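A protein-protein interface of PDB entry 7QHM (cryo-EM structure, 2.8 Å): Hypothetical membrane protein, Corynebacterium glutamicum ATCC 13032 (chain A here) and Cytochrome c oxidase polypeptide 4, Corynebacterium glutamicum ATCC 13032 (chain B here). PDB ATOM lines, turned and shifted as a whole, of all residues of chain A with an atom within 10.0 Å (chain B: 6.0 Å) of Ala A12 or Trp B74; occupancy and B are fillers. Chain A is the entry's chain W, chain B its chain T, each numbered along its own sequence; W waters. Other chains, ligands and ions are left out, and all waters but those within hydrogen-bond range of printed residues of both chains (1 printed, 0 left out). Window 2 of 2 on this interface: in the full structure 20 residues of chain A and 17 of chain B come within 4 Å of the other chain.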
ATOM      1  N   PRO A  11      20.271 -26.875  21.819  1.00  0.00           N
ATOM      2  CA  PRO A  11      19.216 -26.404  20.921  1.00  0.00           C
ATOM      3  C   PRO A  11      19.702 -26.125  19.501  1.00  0.00           C
ATOM      4  O   PRO A  11      20.890 -25.891  19.284  1.00  0.00           O
ATOM      5  CB  PRO A  11      18.744 -25.122  21.610  1.00  0.00           C
ATOM      6  CG  PRO A  11      19.045 -25.346  23.100  1.00  0.00           C
ATOM      7  CD  PRO A  11      19.940 -26.565  23.219  1.00  0.00           C
ATOM      8  N   ALA A  12      18.771 -26.152  18.550  1.00  0.00           N
ATOM      9  CA  ALA A  12      19.109 -26.026  17.143  1.00  0.00           C
ATOM     10  C   ALA A  12      19.538 -24.593  16.821  1.00  0.00           C
ATOM     11  O   ALA A  12      19.158 -23.654  17.524  1.00  0.00           O
ATOM     12  CB  ALA A  12      17.910 -26.431  16.288  1.00  0.00           C
ATOM     13  N   PRO A  13      20.330 -24.393  15.764  1.00  0.00           N
ATOM     14  CA  PRO A  13      20.865 -23.054  15.494  1.00  0.00           C
ATOM     15  C   PRO A  13      19.770 -22.072  15.102  1.00  0.00           C
ATOM     16  O   PRO A  13      18.605 -22.422  14.911  1.00  0.00           O
ATOM     17  CB  PRO A  13      21.854 -23.282  14.347  1.00  0.00           C
ATOM     18  CG  PRO A  13      21.387 -24.508  13.686  1.00  0.00           C
ATOM     19  CD  PRO A  13      20.819 -25.370  14.771  1.00  0.00           C
ATOM     20  N   GLU A  14      20.179 -20.809  14.984  1.00  0.00           N
ATOM     21  CA  GLU A  14      19.229 -19.730  14.740  1.00  0.00           C
ATOM     22  C   GLU A  14      18.779 -19.688  13.285  1.00  0.00           C
ATOM     23  O   GLU A  14      17.600 -19.441  13.007  1.00  0.00           O
ATOM     24  CB  GLU A  14      19.850 -18.393  15.145  1.00  0.00           C
ATOM     25  CG  GLU A  14      20.186 -18.294  16.625  1.00  0.00           C
ATOM     26  CD  GLU A  14      20.933 -17.023  16.969  1.00  0.00           C
ATOM     27  OE1 GLU A  14      21.097 -16.166  16.077  1.00  0.00           O
ATOM     28  OE2 GLU A  14      21.359 -16.881  18.134  1.00  0.00           O
ATOM     29  N   ARG A  15      19.699 -19.916  12.348  1.00  0.00           N
ATOM     30  CA  ARG A  15      19.395 -19.945  10.925  1.00  0.00           C
ATOM     31  C   ARG A  15      19.941 -21.231  10.325  1.00  0.00           C
ATOM     32  O   ARG A  15      20.837 -21.868  10.886  1.00  0.00           O
ATOM     33  CB  ARG A  15      19.981 -18.732  10.190  1.00  0.00           C
ATOM     34  CG  ARG A  15      19.260 -17.420  10.470  1.00  0.00           C
ATOM     35  CD  ARG A  15      19.878 -16.661  11.632  1.00  0.00           C
ATOM     36  NE  ARG A  15      19.199 -15.391  11.867  1.00  0.00           N
ATOM     37  CZ  ARG A  15      18.064 -15.244  12.537  1.00  0.00           C
ATOM     38  NH1 ARG A  15      17.423 -16.280  13.061  1.00  0.00           N
ATOM     39  NH2 ARG A  15      17.553 -14.026  12.687  1.00  0.00           N
ATOM     40  N   MET A  16      19.384 -21.601   9.175  1.00  0.00           N
ATOM     41  CA  MET A  16      19.724 -22.835   8.485  1.00  0.00           C
ATOM     42  C   MET A  16      20.287 -22.514   7.110  1.00  0.00           C
ATOM     43  O   MET A  16      20.112 -21.414   6.584  1.00  0.00           O
ATOM     44  CB  MET A  16      18.509 -23.768   8.364  1.00  0.00           C
ATOM     45  CG  MET A  16      17.182 -23.075   8.087  1.00  0.00           C
ATOM     46  SD  MET A  16      15.855 -24.221   7.638  1.00  0.00           S
ATOM     47  CE  MET A  16      15.798 -25.312   9.059  1.00  0.00           C
ATOM     48  N   HIS A  17      20.966 -23.503   6.534  1.00  0.00           N
ATOM     49  CA  HIS A  17      21.733 -23.316   5.310  1.00  0.00           C
ATOM     50  C   HIS A  17      20.797 -23.090   4.132  1.00  0.00           C
ATOM     51  O   HIS A  17      20.048 -23.991   3.745  1.00  0.00           O
ATOM     52  CB  HIS A  17      22.616 -24.532   5.071  1.00  0.00           C
ATOM     53  CG  HIS A  17      23.603 -24.361   3.958  1.00  0.00           C
ATOM     54  ND1 HIS A  17      24.324 -25.414   3.442  1.00  0.00           N
ATOM     55  CD2 HIS A  17      23.996 -23.263   3.273  1.00  0.00           C
ATOM     56  CE1 HIS A  17      25.112 -24.972   2.479  1.00  0.00           C
ATOM     57  NE2 HIS A  17      24.930 -23.671   2.355  1.00  0.00           N
ATOM     58  N   TYR A  18      20.841 -21.891   3.559  1.00  0.00           N
ATOM     59  CA  TYR A  18      20.164 -21.574   2.309  1.00  0.00           C
ATOM     60  C   TYR A  18      21.209 -21.089   1.320  1.00  0.00           C
ATOM     61  O   TYR A  18      21.858 -20.069   1.558  1.00  0.00           O
ATOM     62  CB  TYR A  18      19.097 -20.493   2.498  1.00  0.00           C
ATOM     63  CG  TYR A  18      17.911 -20.849   3.371  1.00  0.00           C
ATOM     64  CD1 TYR A  18      17.462 -22.157   3.494  1.00  0.00           C
ATOM     65  CD2 TYR A  18      17.230 -19.862   4.061  1.00  0.00           C
ATOM     66  CE1 TYR A  18      16.387 -22.468   4.281  1.00  0.00           C
ATOM     67  CE2 TYR A  18      16.152 -20.165   4.849  1.00  0.00           C
ATOM     68  CZ  TYR A  18      15.732 -21.469   4.956  1.00  0.00           C
ATOM     69  OH  TYR A  18      14.652 -21.770   5.748  1.00  0.00           O
ATOM     70  N   TYR A  22      17.906 -20.612  -3.730  1.00  0.00           N
ATOM     71  CA  TYR A  22      16.894 -21.371  -3.014  1.00  0.00           C
ATOM     72  C   TYR A  22      16.004 -20.418  -2.240  1.00  0.00           C
ATOM     73  O   TYR A  22      16.492 -19.485  -1.599  1.00  0.00           O
ATOM     74  CB  TYR A  22      17.543 -22.363  -2.057  1.00  0.00           C
ATOM     75  CG  TYR A  22      16.563 -23.219  -1.290  1.00  0.00           C
ATOM     76  CD1 TYR A  22      15.732 -24.105  -1.946  1.00  0.00           C
ATOM     77  CD2 TYR A  22      16.483 -23.155   0.086  1.00  0.00           C
ATOM     78  CE1 TYR A  22      14.847 -24.887  -1.259  1.00  0.00           C
ATOM     79  CE2 TYR A  22      15.601 -23.939   0.782  1.00  0.00           C
ATOM     80  CZ  TYR A  22      14.788 -24.804   0.105  1.00  0.00           C
ATOM     81  OH  TYR A  22      13.900 -25.592   0.790  1.00  0.00           O
ATOM     82  N   VAL A  25       9.434 -22.452   1.608  1.00  0.00           N
ATOM     83  CA  VAL A  25       8.139 -22.207   2.231  1.00  0.00           C
ATOM     84  C   VAL A  25       8.374 -22.363   3.728  1.00  0.00           C
ATOM     85  O   VAL A  25       8.501 -23.483   4.227  1.00  0.00           O
ATOM     86  CB  VAL A  25       7.070 -23.176   1.727  1.00  0.00           C
ATOM     87  CG1 VAL A  25       5.725 -22.875   2.380  1.00  0.00           C
ATOM     88  CG2 VAL A  25       6.957 -23.108   0.221  1.00  0.00           C
ATOM     89  N   ALA A  26       8.427 -21.241   4.453  1.00  0.00           N
ATOM     90  CA  ALA A  26       9.034 -21.186   5.782  1.00  0.00           C
ATOM     91  C   ALA A  26       8.062 -20.558   6.780  1.00  0.00           C
ATOM     92  O   ALA A  26       8.302 -19.464   7.292  1.00  0.00           O
ATOM     93  CB  ALA A  26      10.344 -20.413   5.735  1.00  0.00           C
ATOM     94  N   TYR A  27       6.978 -21.272   7.081  1.00  0.00           N
ATOM     95  CA  TYR A  27       6.035 -20.825   8.098  1.00  0.00           C
ATOM     96  C   TYR A  27       6.430 -21.278   9.497  1.00  0.00           C
ATOM     97  O   TYR A  27       6.275 -20.519  10.454  1.00  0.00           O
ATOM     98  CB  TYR A  27       4.632 -21.336   7.779  1.00  0.00           C
ATOM     99  CG  TYR A  27       4.036 -20.740   6.534  1.00  0.00           C
ATOM    100  CD1 TYR A  27       3.744 -19.390   6.465  1.00  0.00           C
ATOM    101  CD2 TYR A  27       3.747 -21.528   5.439  1.00  0.00           C
ATOM    102  CE1 TYR A  27       3.208 -18.844   5.341  1.00  0.00           C
ATOM    103  CE2 TYR A  27       3.203 -20.992   4.312  1.00  0.00           C
ATOM    104  CZ  TYR A  27       2.932 -19.649   4.268  1.00  0.00           C
ATOM    105  OH  TYR A  27       2.390 -19.106   3.133  1.00  0.00           O
ATOM    106  N   SER A  28       6.928 -22.500   9.643  1.00  0.00           N
ATOM    107  CA  SER A  28       7.286 -23.048  10.942  1.00  0.00           C
ATOM    108  C   SER A  28       8.748 -22.803  11.301  1.00  0.00           C
ATOM    109  O   SER A  28       9.292 -23.511  12.154  1.00  0.00           O
ATOM    110  CB  SER A  28       6.983 -24.548  10.977  1.00  0.00           C
ATOM    111  OG  SER A  28       5.600 -24.793  10.804  1.00  0.00           O
ATOM    112  N   SER A  29       9.392 -21.820  10.680  1.00  0.00           N
ATOM    113  CA  SER A  29      10.777 -21.542  10.993  1.00  0.00           C
ATOM    114  C   SER A  29      10.887 -20.982  12.410  1.00  0.00           C
ATOM    115  O   SER A  29       9.889 -20.569  12.997  1.00  0.00           O
ATOM    116  CB  SER A  29      11.364 -20.571   9.977  1.00  0.00           C
ATOM    117  OG  SER A  29      10.449 -19.538   9.684  1.00  0.00           O
ATOM    118  N   PRO A  30      12.091 -20.966  12.992  1.00  0.00           N
ATOM    119  CA  PRO A  30      12.213 -20.491  14.379  1.00  0.00           C
ATOM    120  C   PRO A  30      11.910 -19.018  14.570  1.00  0.00           C
ATOM    121  O   PRO A  30      11.593 -18.617  15.694  1.00  0.00           O
ATOM    122  CB  PRO A  30      13.673 -20.800  14.724  1.00  0.00           C
ATOM    123  CG  PRO A  30      14.061 -21.856  13.777  1.00  0.00           C
ATOM    124  CD  PRO A  30      13.363 -21.532  12.520  1.00  0.00           C
ATOM    125  N   HIS A  31      12.010 -18.200  13.524  1.00  0.00           N
ATOM    126  CA  HIS A  31      11.755 -16.770  13.606  1.00  0.00           C
ATOM    127  C   HIS A  31      10.345 -16.391  13.177  1.00  0.00           C
ATOM    128  O   HIS A  31      10.045 -15.200  13.072  1.00  0.00           O
ATOM    129  CB  HIS A  31      12.760 -16.004  12.747  1.00  0.00           C
ATOM    130  CG  HIS A  31      12.701 -16.353  11.295  1.00  0.00           C
ATOM    131  ND1 HIS A  31      11.768 -15.816  10.435  1.00  0.00           N
ATOM    132  CD2 HIS A  31      13.451 -17.197  10.556  1.00  0.00           C
ATOM    133  CE1 HIS A  31      11.953 -16.309   9.226  1.00  0.00           C
ATOM    134  NE2 HIS A  31      12.969 -17.149   9.272  1.00  0.00           N
ATOM    135  N   GLU A  35       4.612 -19.162  15.906  1.00  0.00           N
ATOM    136  CA  GLU A  35       4.926 -20.020  17.034  1.00  0.00           C
ATOM    137  C   GLU A  35       5.286 -19.258  18.304  1.00  0.00           C
ATOM    138  O   GLU A  35       5.582 -19.898  19.318  1.00  0.00           O
ATOM    139  CB  GLU A  35       6.084 -20.964  16.673  1.00  0.00           C
ATOM    140  CG  GLU A  35       7.375 -20.269  16.227  1.00  0.00           C
ATOM    141  CD  GLU A  35       8.590 -21.159  16.378  1.00  0.00           C
ATOM    142  OE1 GLU A  35       8.580 -22.281  15.831  1.00  0.00           O
ATOM    143  OE2 GLU A  35       9.552 -20.745  17.058  1.00  0.00           O
ATOM    144  N   VAL B  69      14.411 -30.417  19.640  1.00  0.00           N
ATOM    145  CA  VAL B  69      14.022 -29.995  18.300  1.00  0.00           C
ATOM    146  C   VAL B  69      13.883 -31.266  17.469  1.00  0.00           C
ATOM    147  O   VAL B  69      14.877 -31.861  17.056  1.00  0.00           O
ATOM    148  CB  VAL B  69      15.029 -29.018  17.693  1.00  0.00           C
ATOM    149  CG1 VAL B  69      14.629 -28.628  16.264  1.00  0.00           C
ATOM    150  CG2 VAL B  69      15.140 -27.779  18.565  1.00  0.00           C
ATOM    151  N   LEU B  70      12.653 -31.684  17.230  1.00  0.00           N
ATOM    152  CA  LEU B  70      12.408 -32.925  16.522  1.00  0.00           C
ATOM    153  C   LEU B  70      12.471 -32.697  15.019  1.00  0.00           C
ATOM    154  O   LEU B  70      12.289 -31.574  14.548  1.00  0.00           O
ATOM    155  CB  LEU B  70      11.047 -33.491  16.907  1.00  0.00           C
ATOM    156  CG  LEU B  70      10.814 -33.676  18.404  1.00  0.00           C
ATOM    157  CD1 LEU B  70       9.405 -34.177  18.652  1.00  0.00           C
ATOM    158  CD2 LEU B  70      11.834 -34.620  19.008  1.00  0.00           C
ATOM    159  N   PRO B  71      12.734 -33.745  14.236  1.00  0.00           N
ATOM    160  CA  PRO B  71      12.768 -33.548  12.784  1.00  0.00           C
ATOM    161  C   PRO B  71      11.423 -33.167  12.198  1.00  0.00           C
ATOM    162  O   PRO B  71      11.385 -32.411  11.222  1.00  0.00           O
ATOM    163  CB  PRO B  71      13.263 -34.900  12.261  1.00  0.00           C
ATOM    164  CG  PRO B  71      12.999 -35.852  13.343  1.00  0.00           C
ATOM    165  CD  PRO B  71      13.137 -35.112  14.603  1.00  0.00           C
ATOM    166  N   GLU B  72      10.316 -33.649  12.760  1.00  0.00           N
ATOM    167  CA  GLU B  72       9.006 -33.257  12.251  1.00  0.00           C
ATOM    168  C   GLU B  72       8.611 -31.842  12.646  1.00  0.00           C
ATOM    169  O   GLU B  72       7.586 -31.355  12.160  1.00  0.00           O
ATOM    170  CB  GLU B  72       7.926 -34.227  12.722  1.00  0.00           C
ATOM    171  CG  GLU B  72       7.828 -34.405  14.208  1.00  0.00           C
ATOM    172  CD  GLU B  72       8.454 -35.688  14.661  1.00  0.00           C
ATOM    173  OE1 GLU B  72       9.589 -35.989  14.232  1.00  0.00           O
ATOM    174  OE2 GLU B  72       7.805 -36.411  15.446  1.00  0.00           O
ATOM    175  N   ASP B  73       9.379 -31.185  13.512  1.00  0.00           N
ATOM    176  CA  ASP B  73       9.173 -29.791  13.878  1.00  0.00           C
ATOM    177  C   ASP B  73      10.289 -28.910  13.333  1.00  0.00           C
ATOM    178  O   ASP B  73      10.642 -27.897  13.938  1.00  0.00           O
ATOM    179  CB  ASP B  73       9.072 -29.657  15.393  1.00  0.00           C
ATOM    180  CG  ASP B  73       7.905 -30.439  15.975  1.00  0.00           C
ATOM    181  OD1 ASP B  73       7.037 -30.893  15.198  1.00  0.00           O
ATOM    182  OD2 ASP B  73       7.855 -30.605  17.210  1.00  0.00           O
ATOM    183  N   TRP B  74      10.837 -29.283  12.180  1.00  0.00           N
ATOM    184  CA  TRP B  74      12.018 -28.657  11.604  1.00  0.00           C
ATOM    185  C   TRP B  74      11.797 -28.518  10.111  1.00  0.00           C
ATOM    186  O   TRP B  74      11.244 -29.415   9.473  1.00  0.00           O
ATOM    187  CB  TRP B  74      13.266 -29.490  11.894  1.00  0.00           C
ATOM    188  CG  TRP B  74      14.557 -28.819  11.602  1.00  0.00           C
ATOM    189  CD1 TRP B  74      15.496 -29.222  10.710  1.00  0.00           C
ATOM    190  CD2 TRP B  74      15.071 -27.636  12.218  1.00  0.00           C
ATOM    191  NE1 TRP B  74      16.563 -28.363  10.725  1.00  0.00           N
ATOM    192  CE2 TRP B  74      16.326 -27.382  11.648  1.00  0.00           C
ATOM    193  CE3 TRP B  74      14.591 -26.765  13.198  1.00  0.00           C
ATOM    194  CZ2 TRP B  74      17.102 -26.295  12.012  1.00  0.00           C
ATOM    195  CZ3 TRP B  74      15.366 -25.688  13.560  1.00  0.00           C
ATOM    196  CH2 TRP B  74      16.607 -25.463  12.969  1.00  0.00           C
ATOM    197  N   GLU B  75      12.226 -27.391   9.556  1.00  0.00           N
ATOM    198  CA  GLU B  75      11.815 -27.029   8.210  1.00  0.00           C
ATOM    199  C   GLU B  75      12.639 -27.696   7.119  1.00  0.00           C
ATOM    200  O   GLU B  75      12.189 -27.733   5.971  1.00  0.00           O
ATOM    201  CB  GLU B  75      11.889 -25.512   8.045  1.00  0.00           C
ATOM    202  CG  GLU B  75      10.907 -24.737   8.896  1.00  0.00           C
ATOM    203  CD  GLU B  75       9.540 -24.629   8.258  1.00  0.00           C
ATOM    204  OE1 GLU B  75       9.054 -25.644   7.736  1.00  0.00           O
ATOM    205  OE2 GLU B  75       8.953 -23.526   8.271  1.00  0.00           O
ATOM    206  N   GLU B  76      13.822 -28.214   7.439  1.00  0.00           N
ATOM    207  CA  GLU B  76      14.743 -28.804   6.470  1.00  0.00           C
ATOM    208  C   GLU B  76      15.234 -30.155   6.958  1.00  0.00           C
ATOM    209  O   GLU B  76      16.410 -30.498   6.828  1.00  0.00           O
ATOM    210  CB  GLU B  76      15.916 -27.864   6.196  1.00  0.00           C
ATOM    211  CG  GLU B  76      15.575 -26.693   5.308  1.00  0.00           C
ATOM    212  CD  GLU B  76      15.369 -27.091   3.870  1.00  0.00           C
ATOM    213  OE1 GLU B  76      15.750 -28.213   3.493  1.00  0.00           O
ATOM    214  OE2 GLU B  76      14.822 -26.274   3.106  1.00  0.00           O
ATOM    215  N   ALA B  77      14.330 -30.948   7.518  1.00  0.00           N
ATOM    216  CA  ALA B  77      14.684 -32.261   8.023  1.00  0.00           C
ATOM    217  C   ALA B  77      14.880 -33.244   6.882  1.00  0.00           C
ATOM    218  O   ALA B  77      14.146 -33.225   5.892  1.00  0.00           O
ATOM    219  CB  ALA B  77      13.601 -32.775   8.965  1.00  0.00           C
HETATM  220  O   HOH W   1       6.493 -24.716   6.216  1.00  0.00           O
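OH of Tyr A22 lies within hydrogen-bond range of OE2 of Glu B76, 2.6 Å away. The backbone NH of Tyr A27 lies within hydrogen-bond range of the side-chain carboxylate of Glu B75. N of Ser A28 is in hydrogen-bond range of OE2 of Glu B75 (2.7 Å). N of Ser A29 sits at hydrogen-bond distance from OE2 of Glu B75, at 3.0 Å.
The side-chain sulfur (SD) of Met A16 sits at hydrogen-bond distance from the side-chain hydroxyl (OH) of Tyr A18. OG of Ser A29 is in hydrogen-bond range of O of Ala A26, at 3.2 Å. The side-chain hydroxyl (OG) of Ser A29 lies within hydrogen-bond range of a ring nitrogen (NE2) of His A31.
Val B69 touches Ala A12 (CG2 to CB, 3.8 Å). Ala A12 touches Trp B74 (CB to CH2, 3.7 Å). CE of Met A16 touches CE2 of Trp B74, 3.4 Å away. Met A16 touches Glu B76. Glu B75 touches Ala A26 (OE2 to CA, 3.4 Å).
Of the printed residues of chain B, Ala A12 touches Val B69 (3.8 Å) and Trp B74 (3.7 Å). Printed residues of chain B within 4 Å of Tyr A22: Glu B76. Glu A35 touches none of the printed residues of chain B. Asp B73 touches none of the printed residues of chain A. Trp B74 touches just these residues of chain A: Ala A12 and Met A16. Of the printed residues of chain A, Glu B75 touches Ala A26 (3.4 Å), Tyr A27 (3.2 Å), Ser A28 (2.7 Å) and Ser A29 (3.0 Å). Printed residues of chain A within 4 Å of Glu B76: Met A16 and Tyr A22. The nearest residue of chain A that does not touch Trp B74 is Pro A30 (4.1 Å).
Of the 9 printed residues of chain B, 4 touch a printed residue of chain A.
Water W1 bridges O of Val A25 (3.1 Å) and OE1 of Glu B75 (3.1 Å).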
